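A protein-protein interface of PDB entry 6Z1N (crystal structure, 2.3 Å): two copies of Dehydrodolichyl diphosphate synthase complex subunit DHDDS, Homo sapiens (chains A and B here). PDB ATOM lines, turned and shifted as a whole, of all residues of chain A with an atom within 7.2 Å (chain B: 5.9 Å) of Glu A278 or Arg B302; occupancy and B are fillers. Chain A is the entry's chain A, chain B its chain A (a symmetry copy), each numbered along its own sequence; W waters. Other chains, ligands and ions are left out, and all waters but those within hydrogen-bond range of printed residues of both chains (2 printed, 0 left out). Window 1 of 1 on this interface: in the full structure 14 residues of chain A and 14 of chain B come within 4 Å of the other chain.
The side-chain carboxylate of Glu A271 is in salt-bridge range of the guanidinium group of Arg B303 (2.8 Å). The side-chain amide oxygen of Gln A275 lies close to the backbone carbonyl oxygen of Ser B296, at 2.6 Å. The side-chain carboxylate (OE2) of Glu A278 is in salt-bridge range of the guanidinium group (NE) of Arg B303.
The guanidinium group of Arg A272 is in hydrogen-bond range of the side-chain amide oxygen of Gln A275, 3.1 Å away. The backbone carbonyl oxygen (O) of Arg A279 lies within hydrogen-bond range of the side-chain hydroxyl (OG1) of Thr A283 (3.1 Å). The backbone carbonyl oxygen of Gln A281 lies within hydrogen-bond range of the side-chain hydroxyl of Thr A285 (2.9 Å). The side-chain amide oxygen of Gln B281 lies within hydrogen-bond range of the guanidinium group of Arg B302, 3.0 Å away. The guanidinium group (NH2) of Arg B302 lies within hydrogen-bond range of the side-chain hydroxyl (OG1) of Thr B285, at 2.4 Å. The backbone carbonyl oxygen (O) of Ala B295 is in hydrogen-bond range of the guanidinium group (NE) of Arg B302, 3.4 Å away.
Arg A274 touches Arg B303. Gln A275 touches Gly B297 (NE2 to O, 3.5 Å). CG of Gln A275 touches NH2 of Arg B303, 3.7 Å away. Glu A278 touches Ala B295. CD of Glu A278 touches CD of Arg B302, 3.5 Å away. CD of Arg A279 touches CB of Ser B296, at 3.7 Å. Ala A282 touches Thr B285 (CB to CG2, 3.7 Å). CB of Ala B282 touches CG2 of Thr A285, 3.7 Å away.
Glu A278 touches three residues of chain B. Printed residues of chain B within 4 Å of Arg A279: Ser B296. Asp A280 touches none of the printed residues of chain B. Of the printed residues of chain B, Thr A285 touches Ala B282 (3.7 Å). Of the printed residues of chain A, Ala B295 touches Glu A278. Arg B302 touches just one residue of chain A: Glu A278. The nearest residue of chain A that does not touch Arg B302 is Ala A282 (4.3 Å). The nearest printed residue of chain B that does not touch Thr A285 is Thr B285 (5.0 Å).
Of the 15 printed residues of chain A, 7 touch a printed residue of chain B. Hydrophobic or aromatic side chains of chain A within 4 Å of the printed part of chain B: Ala A282. Printed residues of chain B that touch a printed residue of chain A: Ala B282, Thr B285, Ala B295, Ser B296, Gly B297, Arg B302 and Arg B303. Hydrophobic or aromatic side chains of chain B that line the printed part of chain A: Ala B282. Among the printed residues, 11 pairs touch across the chains. Among the printed residues, Asp or Glu carboxylates within 4 Å of a Lys or Arg side-chain nitrogen of the other chain: Glu A271 with Arg B303 and Glu A278 with Arg B303.
Ala A282 touches Thr B285, and with the chains exchanged Thr A285 touches Ala B282. Positions printed for both chains: 280, 281, 282, 284 and 285. Of the 11 pairs that touch across the chains among the printed residues, 2 have their exchanged pair printed and touching as well.
Water W1 lies within hydrogen-bond range of the backbone carbonyl oxygen (O) of Glu A278 and the guanidinium group (NH2) of Arg B302. Water W2 bridges the side-chain hydroxyl (OG1) of Thr A285 and the side-chain hydroxyl (OG1) of Thr B285.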
ATOM      1  N   GLU A 271     -32.441 -13.789   1.997  1.00  0.00           N
ATOM      2  CA  GLU A 271     -31.153 -14.102   1.391  1.00  0.00           C
ATOM      3  C   GLU A 271     -30.795 -13.091   0.312  1.00  0.00           C
ATOM      4  O   GLU A 271     -29.632 -12.696   0.191  1.00  0.00           O
ATOM      5  CB  GLU A 271     -31.155 -15.522   0.825  1.00  0.00           C
ATOM      6  CG  GLU A 271     -29.855 -15.914   0.133  1.00  0.00           C
ATOM      7  CD  GLU A 271     -28.652 -15.886   1.065  1.00  0.00           C
ATOM      8  OE1 GLU A 271     -28.845 -16.000   2.295  1.00  0.00           O
ATOM      9  OE2 GLU A 271     -27.511 -15.744   0.567  1.00  0.00           O
ATOM     10  N   ARG A 272     -31.784 -12.645  -0.467  1.00  0.00           N
ATOM     11  CA  ARG A 272     -31.518 -11.626  -1.480  1.00  0.00           C
ATOM     12  C   ARG A 272     -31.061 -10.322  -0.840  1.00  0.00           C
ATOM     13  O   ARG A 272     -30.093  -9.703  -1.302  1.00  0.00           O
ATOM     14  CB  ARG A 272     -32.760 -11.393  -2.341  1.00  0.00           C
ATOM     15  CG  ARG A 272     -33.190 -12.602  -3.192  1.00  0.00           C
ATOM     16  CD  ARG A 272     -32.009 -13.335  -3.828  1.00  0.00           C
ATOM     17  NE  ARG A 272     -31.223 -12.457  -4.691  1.00  0.00           N
ATOM     18  CZ  ARG A 272     -30.104 -12.822  -5.312  1.00  0.00           C
ATOM     19  NH1 ARG A 272     -29.446 -11.951  -6.070  1.00  0.00           N
ATOM     20  NH2 ARG A 272     -29.642 -14.056  -5.173  1.00  0.00           N
ATOM     21  N   LYS A 273     -31.736  -9.892   0.234  1.00  0.00           N
ATOM     22  CA  LYS A 273     -31.315  -8.672   0.919  1.00  0.00           C
ATOM     23  C   LYS A 273     -29.929  -8.845   1.530  1.00  0.00           C
ATOM     24  O   LYS A 273     -29.098  -7.929   1.472  1.00  0.00           O
ATOM     25  CB  LYS A 273     -32.339  -8.273   1.991  1.00  0.00           C
ATOM     26  N   ARG A 274     -29.656 -10.020   2.103  1.00  0.00           N
ATOM     27  CA  ARG A 274     -28.330 -10.285   2.651  1.00  0.00           C
ATOM     28  C   ARG A 274     -27.255 -10.127   1.580  1.00  0.00           C
ATOM     29  O   ARG A 274     -26.270  -9.408   1.776  1.00  0.00           O
ATOM     30  CB  ARG A 274     -28.292 -11.685   3.264  1.00  0.00           C
ATOM     31  CG  ARG A 274     -27.007 -12.020   4.001  1.00  0.00           C
ATOM     32  CD  ARG A 274     -27.171 -13.272   4.850  1.00  0.00           C
ATOM     33  N   GLN A 275     -27.450 -10.766   0.423  1.00  0.00           N
ATOM     34  CA  GLN A 275     -26.463 -10.688  -0.651  1.00  0.00           C
ATOM     35  C   GLN A 275     -26.372  -9.284  -1.235  1.00  0.00           C
ATOM     36  O   GLN A 275     -25.295  -8.862  -1.670  1.00  0.00           O
ATOM     37  CB  GLN A 275     -26.799 -11.699  -1.748  1.00  0.00           C
ATOM     38  CG  GLN A 275     -26.729 -13.160  -1.303  1.00  0.00           C
ATOM     39  CD  GLN A 275     -26.940 -14.130  -2.455  1.00  0.00           C
ATOM     40  OE1 GLN A 275     -26.957 -13.727  -3.613  1.00  0.00           O
ATOM     41  NE2 GLN A 275     -27.138 -15.410  -2.137  1.00  0.00           N
ATOM     42  N   GLN A 276     -27.485  -8.551  -1.264  1.00  0.00           N
ATOM     43  CA  GLN A 276     -27.438  -7.163  -1.705  1.00  0.00           C
ATOM     44  C   GLN A 276     -26.625  -6.309  -0.740  1.00  0.00           C
ATOM     45  O   GLN A 276     -25.897  -5.401  -1.167  1.00  0.00           O
ATOM     46  CB  GLN A 276     -28.857  -6.607  -1.844  1.00  0.00           C
ATOM     47  CG  GLN A 276     -28.903  -5.199  -2.424  1.00  0.00           C
ATOM     48  CD  GLN A 276     -28.281  -5.134  -3.803  1.00  0.00           C
ATOM     49  OE1 GLN A 276     -27.260  -4.478  -4.002  1.00  0.00           O
ATOM     50  NE2 GLN A 276     -28.888  -5.824  -4.763  1.00  0.00           N
ATOM     51  N   LEU A 277     -26.738  -6.576   0.566  1.00  0.00           N
ATOM     52  CA  LEU A 277     -25.913  -5.847   1.526  1.00  0.00           C
ATOM     53  C   LEU A 277     -24.442  -6.199   1.351  1.00  0.00           C
ATOM     54  O   LEU A 277     -23.584  -5.308   1.348  1.00  0.00           O
ATOM     55  CB  LEU A 277     -26.375  -6.129   2.956  1.00  0.00           C
ATOM     56  CG  LEU A 277     -25.519  -5.518   4.073  1.00  0.00           C
ATOM     57  CD1 LEU A 277     -25.435  -4.003   3.953  1.00  0.00           C
ATOM     58  CD2 LEU A 277     -26.073  -5.904   5.441  1.00  0.00           C
ATOM     59  N   GLU A 278     -24.138  -7.492   1.181  1.00  0.00           N
ATOM     60  CA  GLU A 278     -22.759  -7.907   0.940  1.00  0.00           C
ATOM     61  C   GLU A 278     -22.191  -7.221  -0.295  1.00  0.00           C
ATOM     62  O   GLU A 278     -21.045  -6.752  -0.283  1.00  0.00           O
ATOM     63  CB  GLU A 278     -22.684  -9.429   0.794  1.00  0.00           C
ATOM     64  CG  GLU A 278     -22.762 -10.196   2.110  1.00  0.00           C
ATOM     65  CD  GLU A 278     -23.078 -11.675   1.917  1.00  0.00           C
ATOM     66  OE1 GLU A 278     -23.382 -12.080   0.775  1.00  0.00           O
ATOM     67  OE2 GLU A 278     -23.016 -12.437   2.907  1.00  0.00           O
ATOM     68  N   ARG A 279     -22.987  -7.136  -1.366  1.00  0.00           N
ATOM     69  CA  ARG A 279     -22.521  -6.514  -2.604  1.00  0.00           C
ATOM     70  C   ARG A 279     -22.259  -5.025  -2.405  1.00  0.00           C
ATOM     71  O   ARG A 279     -21.243  -4.495  -2.865  1.00  0.00           O
ATOM     72  CB  ARG A 279     -23.547  -6.735  -3.719  1.00  0.00           C
ATOM     73  CG  ARG A 279     -22.957  -7.229  -5.031  1.00  0.00           C
ATOM     74  CD  ARG A 279     -23.980  -8.020  -5.832  1.00  0.00           C
ATOM     75  N   ASP A 280     -23.176  -4.334  -1.722  1.00  0.00           N
ATOM     76  CA  ASP A 280     -22.991  -2.908  -1.476  1.00  0.00           C
ATOM     77  C   ASP A 280     -21.782  -2.650  -0.577  1.00  0.00           C
ATOM     78  O   ASP A 280     -21.030  -1.696  -0.806  1.00  0.00           O
ATOM     79  CB  ASP A 280     -24.264  -2.308  -0.870  1.00  0.00           C
ATOM     80  CG  ASP A 280     -25.455  -2.352  -1.834  1.00  0.00           C
ATOM     81  OD1 ASP A 280     -25.236  -2.338  -3.064  1.00  0.00           O
ATOM     82  OD2 ASP A 280     -26.611  -2.403  -1.360  1.00  0.00           O
ATOM     83  N   GLN A 281     -21.574  -3.492   0.443  1.00  0.00           N
ATOM     84  CA  GLN A 281     -20.381  -3.353   1.277  1.00  0.00           C
ATOM     85  C   GLN A 281     -19.110  -3.546   0.459  1.00  0.00           C
ATOM     86  O   GLN A 281     -18.109  -2.856   0.686  1.00  0.00           O
ATOM     87  CB  GLN A 281     -20.417  -4.349   2.437  1.00  0.00           C
ATOM     88  CG  GLN A 281     -21.586  -4.180   3.389  1.00  0.00           C
ATOM     89  CD  GLN A 281     -21.316  -3.157   4.475  1.00  0.00           C
ATOM     90  OE1 GLN A 281     -20.574  -2.196   4.269  1.00  0.00           O
ATOM     91  NE2 GLN A 281     -21.931  -3.352   5.635  1.00  0.00           N
ATOM     92  N   ALA A 282     -19.126  -4.484  -0.500  1.00  0.00           N
ATOM     93  CA  ALA A 282     -17.938  -4.722  -1.320  1.00  0.00           C
ATOM     94  C   ALA A 282     -17.668  -3.547  -2.248  1.00  0.00           C
ATOM     95  O   ALA A 282     -16.511  -3.154  -2.439  1.00  0.00           O
ATOM     96  CB  ALA A 282     -18.090  -6.016  -2.118  1.00  0.00           C
ATOM     97  N   THR A 283     -18.725  -2.971  -2.825  1.00  0.00           N
ATOM     98  CA  THR A 283     -18.594  -1.736  -3.594  1.00  0.00           C
ATOM     99  C   THR A 283     -17.942  -0.633  -2.767  1.00  0.00           C
ATOM    100  O   THR A 283     -16.957  -0.016  -3.194  1.00  0.00           O
ATOM    101  CB  THR A 283     -19.972  -1.288  -4.084  1.00  0.00           C
ATOM    102  OG1 THR A 283     -20.540  -2.317  -4.903  1.00  0.00           O
ATOM    103  CG2 THR A 283     -19.874   0.010  -4.880  1.00  0.00           C
ATOM    104  N   VAL A 284     -18.483  -0.375  -1.572  1.00  0.00           N
ATOM    105  CA  VAL A 284     -17.937   0.664  -0.703  1.00  0.00           C
ATOM    106  C   VAL A 284     -16.485   0.360  -0.354  1.00  0.00           C
ATOM    107  O   VAL A 284     -15.645   1.263  -0.290  1.00  0.00           O
ATOM    108  CB  VAL A 284     -18.802   0.817   0.565  1.00  0.00           C
ATOM    109  CG1 VAL A 284     -18.156   1.800   1.542  1.00  0.00           C
ATOM    110  CG2 VAL A 284     -20.218   1.254   0.214  1.00  0.00           C
ATOM    111  N   THR A 285     -16.163  -0.919  -0.131  1.00  0.00           N
ATOM    112  CA  THR A 285     -14.782  -1.289   0.167  1.00  0.00           C
ATOM    113  C   THR A 285     -13.869  -0.980  -1.011  1.00  0.00           C
ATOM    114  O   THR A 285     -12.773  -0.436  -0.831  1.00  0.00           O
ATOM    115  CB  THR A 285     -14.691  -2.775   0.537  1.00  0.00           C
ATOM    116  OG1 THR A 285     -15.408  -3.021   1.753  1.00  0.00           O
ATOM    117  CG2 THR A 285     -13.236  -3.206   0.721  1.00  0.00           C
ATOM    118  N   ASP B 280     -12.493  -7.954   8.388  1.00  0.00           N
ATOM    119  CA  ASP B 280     -12.410  -9.320   7.881  1.00  0.00           C
ATOM    120  C   ASP B 280     -13.229  -9.489   6.602  1.00  0.00           C
ATOM    121  O   ASP B 280     -12.791 -10.174   5.670  1.00  0.00           O
ATOM    122  CB  ASP B 280     -12.862 -10.311   8.958  1.00  0.00           C
ATOM    123  CG  ASP B 280     -11.931 -10.326  10.176  1.00  0.00           C
ATOM    124  OD1 ASP B 280     -10.730 -10.018  10.021  1.00  0.00           O
ATOM    125  OD2 ASP B 280     -12.403 -10.644  11.290  1.00  0.00           O
ATOM    126  N   GLN B 281     -14.414  -8.869   6.534  1.00  0.00           N
ATOM    127  CA  GLN B 281     -15.195  -8.915   5.299  1.00  0.00           C
ATOM    128  C   GLN B 281     -14.445  -8.263   4.145  1.00  0.00           C
ATOM    129  O   GLN B 281     -14.511  -8.742   3.006  1.00  0.00           O
ATOM    130  CB  GLN B 281     -16.551  -8.234   5.497  1.00  0.00           C
ATOM    131  CG  GLN B 281     -17.438  -8.870   6.551  1.00  0.00           C
ATOM    132  CD  GLN B 281     -18.265 -10.019   6.008  1.00  0.00           C
ATOM    133  OE1 GLN B 281     -17.848 -10.717   5.083  1.00  0.00           O
ATOM    134  NE2 GLN B 281     -19.438 -10.229   6.592  1.00  0.00           N
ATOM    135  N   ALA B 282     -13.723  -7.165   4.415  1.00  0.00           N
ATOM    136  CA  ALA B 282     -12.980  -6.490   3.351  1.00  0.00           C
ATOM    137  C   ALA B 282     -11.811  -7.338   2.876  1.00  0.00           C
ATOM    138  O   ALA B 282     -11.537  -7.406   1.671  1.00  0.00           O
ATOM    139  CB  ALA B 282     -12.495  -5.120   3.825  1.00  0.00           C
ATOM    140  N   VAL B 284     -11.750 -10.681   2.936  1.00  0.00           N
ATOM    141  CA  VAL B 284     -12.361 -11.735   2.130  1.00  0.00           C
ATOM    142  C   VAL B 284     -12.772 -11.194   0.766  1.00  0.00           C
ATOM    143  O   VAL B 284     -12.631 -11.875  -0.255  1.00  0.00           O
ATOM    144  CB  VAL B 284     -13.560 -12.356   2.876  1.00  0.00           C
ATOM    145  CG1 VAL B 284     -14.290 -13.358   1.981  1.00  0.00           C
ATOM    146  CG2 VAL B 284     -13.117 -13.014   4.176  1.00  0.00           C
ATOM    147  N   THR B 285     -13.280  -9.958   0.724  1.00  0.00           N
ATOM    148  CA  THR B 285     -13.656  -9.360  -0.554  1.00  0.00           C
ATOM    149  C   THR B 285     -12.440  -9.186  -1.453  1.00  0.00           C
ATOM    150  O   THR B 285     -12.494  -9.495  -2.650  1.00  0.00           O
ATOM    151  CB  THR B 285     -14.352  -8.012  -0.334  1.00  0.00           C
ATOM    152  OG1 THR B 285     -15.592  -8.209   0.358  1.00  0.00           O
ATOM    153  CG2 THR B 285     -14.631  -7.314  -1.665  1.00  0.00           C
ATOM    154  N   LEU B 288     -11.295 -12.238  -2.955  1.00  0.00           N
ATOM    155  CA  LEU B 288     -12.287 -12.781  -3.877  1.00  0.00           C
ATOM    156  C   LEU B 288     -12.306 -12.052  -5.215  1.00  0.00           C
ATOM    157  O   LEU B 288     -12.544 -12.685  -6.248  1.00  0.00           O
ATOM    158  CB  LEU B 288     -13.677 -12.724  -3.245  1.00  0.00           C
ATOM    159  CG  LEU B 288     -14.067 -13.876  -2.323  1.00  0.00           C
ATOM    160  CD1 LEU B 288     -15.541 -13.793  -1.947  1.00  0.00           C
ATOM    161  CD2 LEU B 288     -13.751 -15.198  -2.989  1.00  0.00           C
ATOM    162  N   GLN B 294     -16.826 -14.308  -7.060  1.00  0.00           N
ATOM    163  CA  GLN B 294     -17.761 -13.249  -6.704  1.00  0.00           C
ATOM    164  C   GLN B 294     -18.094 -13.317  -5.218  1.00  0.00           C
ATOM    165  O   GLN B 294     -17.752 -14.277  -4.522  1.00  0.00           O
ATOM    166  CB  GLN B 294     -19.035 -13.341  -7.549  1.00  0.00           C
ATOM    167  CG  GLN B 294     -18.767 -13.129  -9.024  1.00  0.00           C
ATOM    168  CD  GLN B 294     -19.606 -12.025  -9.609  1.00  0.00           C
ATOM    169  OE1 GLN B 294     -20.778 -11.875  -9.265  1.00  0.00           O
ATOM    170  NE2 GLN B 294     -19.006 -11.228 -10.484  1.00  0.00           N
ATOM    171  N   ALA B 295     -18.783 -12.279  -4.733  1.00  0.00           N
ATOM    172  CA  ALA B 295     -19.036 -12.117  -3.307  1.00  0.00           C
ATOM    173  C   ALA B 295     -20.481 -12.349  -2.889  1.00  0.00           C
ATOM    174  O   ALA B 295     -20.747 -12.467  -1.689  1.00  0.00           O
ATOM    175  CB  ALA B 295     -18.616 -10.712  -2.854  1.00  0.00           C
ATOM    176  N   SER B 296     -21.420 -12.407  -3.824  1.00  0.00           N
ATOM    177  CA  SER B 296     -22.837 -12.496  -3.500  1.00  0.00           C
ATOM    178  C   SER B 296     -23.457 -13.747  -4.104  1.00  0.00           C
ATOM    179  O   SER B 296     -24.561 -13.714  -4.649  1.00  0.00           O
ATOM    180  CB  SER B 296     -23.579 -11.246  -3.972  1.00  0.00           C
ATOM    181  N   GLY B 297     -22.761 -14.871  -4.018  1.00  0.00           N
ATOM    182  CA  GLY B 297     -23.243 -16.094  -4.620  1.00  0.00           C
ATOM    183  C   GLY B 297     -24.114 -16.928  -3.693  1.00  0.00           C
ATOM    184  O   GLY B 297     -23.964 -16.899  -2.471  1.00  0.00           O
ATOM    185  N   GLN B 300     -22.462 -19.121  -1.160  1.00  0.00           N
ATOM    186  CA  GLN B 300     -22.044 -18.580   0.132  1.00  0.00           C
ATOM    187  C   GLN B 300     -20.532 -18.701   0.304  1.00  0.00           C
ATOM    188  O   GLN B 300     -20.028 -19.017   1.385  1.00  0.00           O
ATOM    189  CB  GLN B 300     -22.792 -19.254   1.285  1.00  0.00           C
ATOM    190  CG  GLN B 300     -24.285 -18.934   1.308  1.00  0.00           C
ATOM    191  N   LEU B 301     -19.808 -18.448  -0.792  1.00  0.00           N
ATOM    192  CA  LEU B 301     -18.352 -18.539  -0.778  1.00  0.00           C
ATOM    193  C   LEU B 301     -17.751 -17.556   0.220  1.00  0.00           C
ATOM    194  O   LEU B 301     -16.899 -17.924   1.039  1.00  0.00           O
ATOM    195  CB  LEU B 301     -17.811 -18.287  -2.187  1.00  0.00           C
ATOM    196  CG  LEU B 301     -16.450 -18.895  -2.527  1.00  0.00           C
ATOM    197  CD1 LEU B 301     -16.412 -20.368  -2.139  1.00  0.00           C
ATOM    198  CD2 LEU B 301     -16.158 -18.737  -4.009  1.00  0.00           C
ATOM    199  N   ARG B 302     -18.192 -16.295   0.164  1.00  0.00           N
ATOM    200  CA  ARG B 302     -17.743 -15.297   1.129  1.00  0.00           C
ATOM    201  C   ARG B 302     -17.916 -15.796   2.556  1.00  0.00           C
ATOM    202  O   ARG B 302     -17.020 -15.644   3.393  1.00  0.00           O
ATOM    203  CB  ARG B 302     -18.516 -13.990   0.927  1.00  0.00           C
ATOM    204  CG  ARG B 302     -18.747 -13.206   2.217  1.00  0.00           C
ATOM    205  CD  ARG B 302     -19.574 -11.954   1.979  1.00  0.00           C
ATOM    206  NE  ARG B 302     -19.009 -11.135   0.913  1.00  0.00           N
ATOM    207  CZ  ARG B 302     -17.899 -10.414   1.029  1.00  0.00           C
ATOM    208  NH1 ARG B 302     -17.231 -10.389   2.174  1.00  0.00           N
ATOM    209  NH2 ARG B 302     -17.466  -9.703  -0.004  1.00  0.00           N
ATOM    210  N   ARG B 303     -19.058 -16.412   2.849  1.00  0.00           N
ATOM    211  CA  ARG B 303     -19.332 -16.814   4.221  1.00  0.00           C
ATOM    212  C   ARG B 303     -18.457 -17.992   4.640  1.00  0.00           C
ATOM    213  O   ARG B 303     -17.979 -18.037   5.781  1.00  0.00           O
ATOM    214  CB  ARG B 303     -20.821 -17.123   4.370  1.00  0.00           C
ATOM    215  CG  ARG B 303     -21.692 -15.902   4.067  1.00  0.00           C
ATOM    216  CD  ARG B 303     -23.131 -16.273   3.791  1.00  0.00           C
ATOM    217  NE  ARG B 303     -23.816 -15.248   3.012  1.00  0.00           N
ATOM    218  CZ  ARG B 303     -25.130 -15.217   2.809  1.00  0.00           C
ATOM    219  NH1 ARG B 303     -25.905 -16.157   3.334  1.00  0.00           N
ATOM    220  NH2 ARG B 303     -25.667 -14.250   2.080  1.00  0.00           N
ATOM    221  N   THR B 304     -18.209 -18.940   3.728  1.00  0.00           N
ATOM    222  CA  THR B 304     -17.276 -20.022   4.035  1.00  0.00           C
ATOM    223  C   THR B 304     -15.859 -19.484   4.243  1.00  0.00           C
ATOM    224  O   THR B 304     -15.178 -19.865   5.202  1.00  0.00           O
ATOM    225  CB  THR B 304     -17.304 -21.084   2.929  1.00  0.00           C
ATOM    226  N   ARG B 305     -15.403 -18.577   3.372  1.00  0.00           N
ATOM    227  CA  ARG B 305     -14.058 -18.028   3.524  1.00  0.00           C
ATOM    228  C   ARG B 305     -13.932 -17.168   4.783  1.00  0.00           C
ATOM    229  O   ARG B 305     -12.870 -17.154   5.417  1.00  0.00           O
ATOM    230  CB  ARG B 305     -13.676 -17.225   2.279  1.00  0.00           C
ATOM    231  N   LEU B 306     -14.999 -16.457   5.166  1.00  0.00           N
ATOM    232  CA  LEU B 306     -14.964 -15.668   6.396  1.00  0.00           C
ATOM    233  C   LEU B 306     -14.858 -16.565   7.626  1.00  0.00           C
ATOM    234  O   LEU B 306     -14.132 -16.243   8.573  1.00  0.00           O
ATOM    235  CB  LEU B 306     -16.206 -14.771   6.482  1.00  0.00           C
ATOM    236  CG  LEU B 306     -16.291 -13.756   7.627  1.00  0.00           C
ATOM    237  CD1 LEU B 306     -15.237 -12.662   7.485  1.00  0.00           C
ATOM    238  CD2 LEU B 306     -17.684 -13.144   7.705  1.00  0.00           C
ATOM    239  N   HIS B 307     -15.568 -17.695   7.627  1.00  0.00           N
ATOM    240  CA  HIS B 307     -15.495 -18.623   8.753  1.00  0.00           C
ATOM    241  C   HIS B 307     -14.121 -19.277   8.848  1.00  0.00           C
ATOM    242  O   HIS B 307     -13.588 -19.456   9.948  1.00  0.00           O
ATOM    243  CB  HIS B 307     -16.590 -19.682   8.624  1.00  0.00           C
ATOM    244  CG  HIS B 307     -16.421 -20.849   9.547  1.00  0.00           C
ATOM    245  ND1 HIS B 307     -16.982 -20.886  10.806  1.00  0.00           N
ATOM    246  CD2 HIS B 307     -15.774 -22.028   9.388  1.00  0.00           C
ATOM    247  CE1 HIS B 307     -16.677 -22.034  11.388  1.00  0.00           C
ATOM    248  NE2 HIS B 307     -15.944 -22.744  10.548  1.00  0.00           N
HETATM  249  O   HOH W   1     -19.206  -7.687   1.448  1.00  0.00           O
HETATM  250  O   HOH W   2     -16.504  -5.843   2.035  1.00  0.00           O
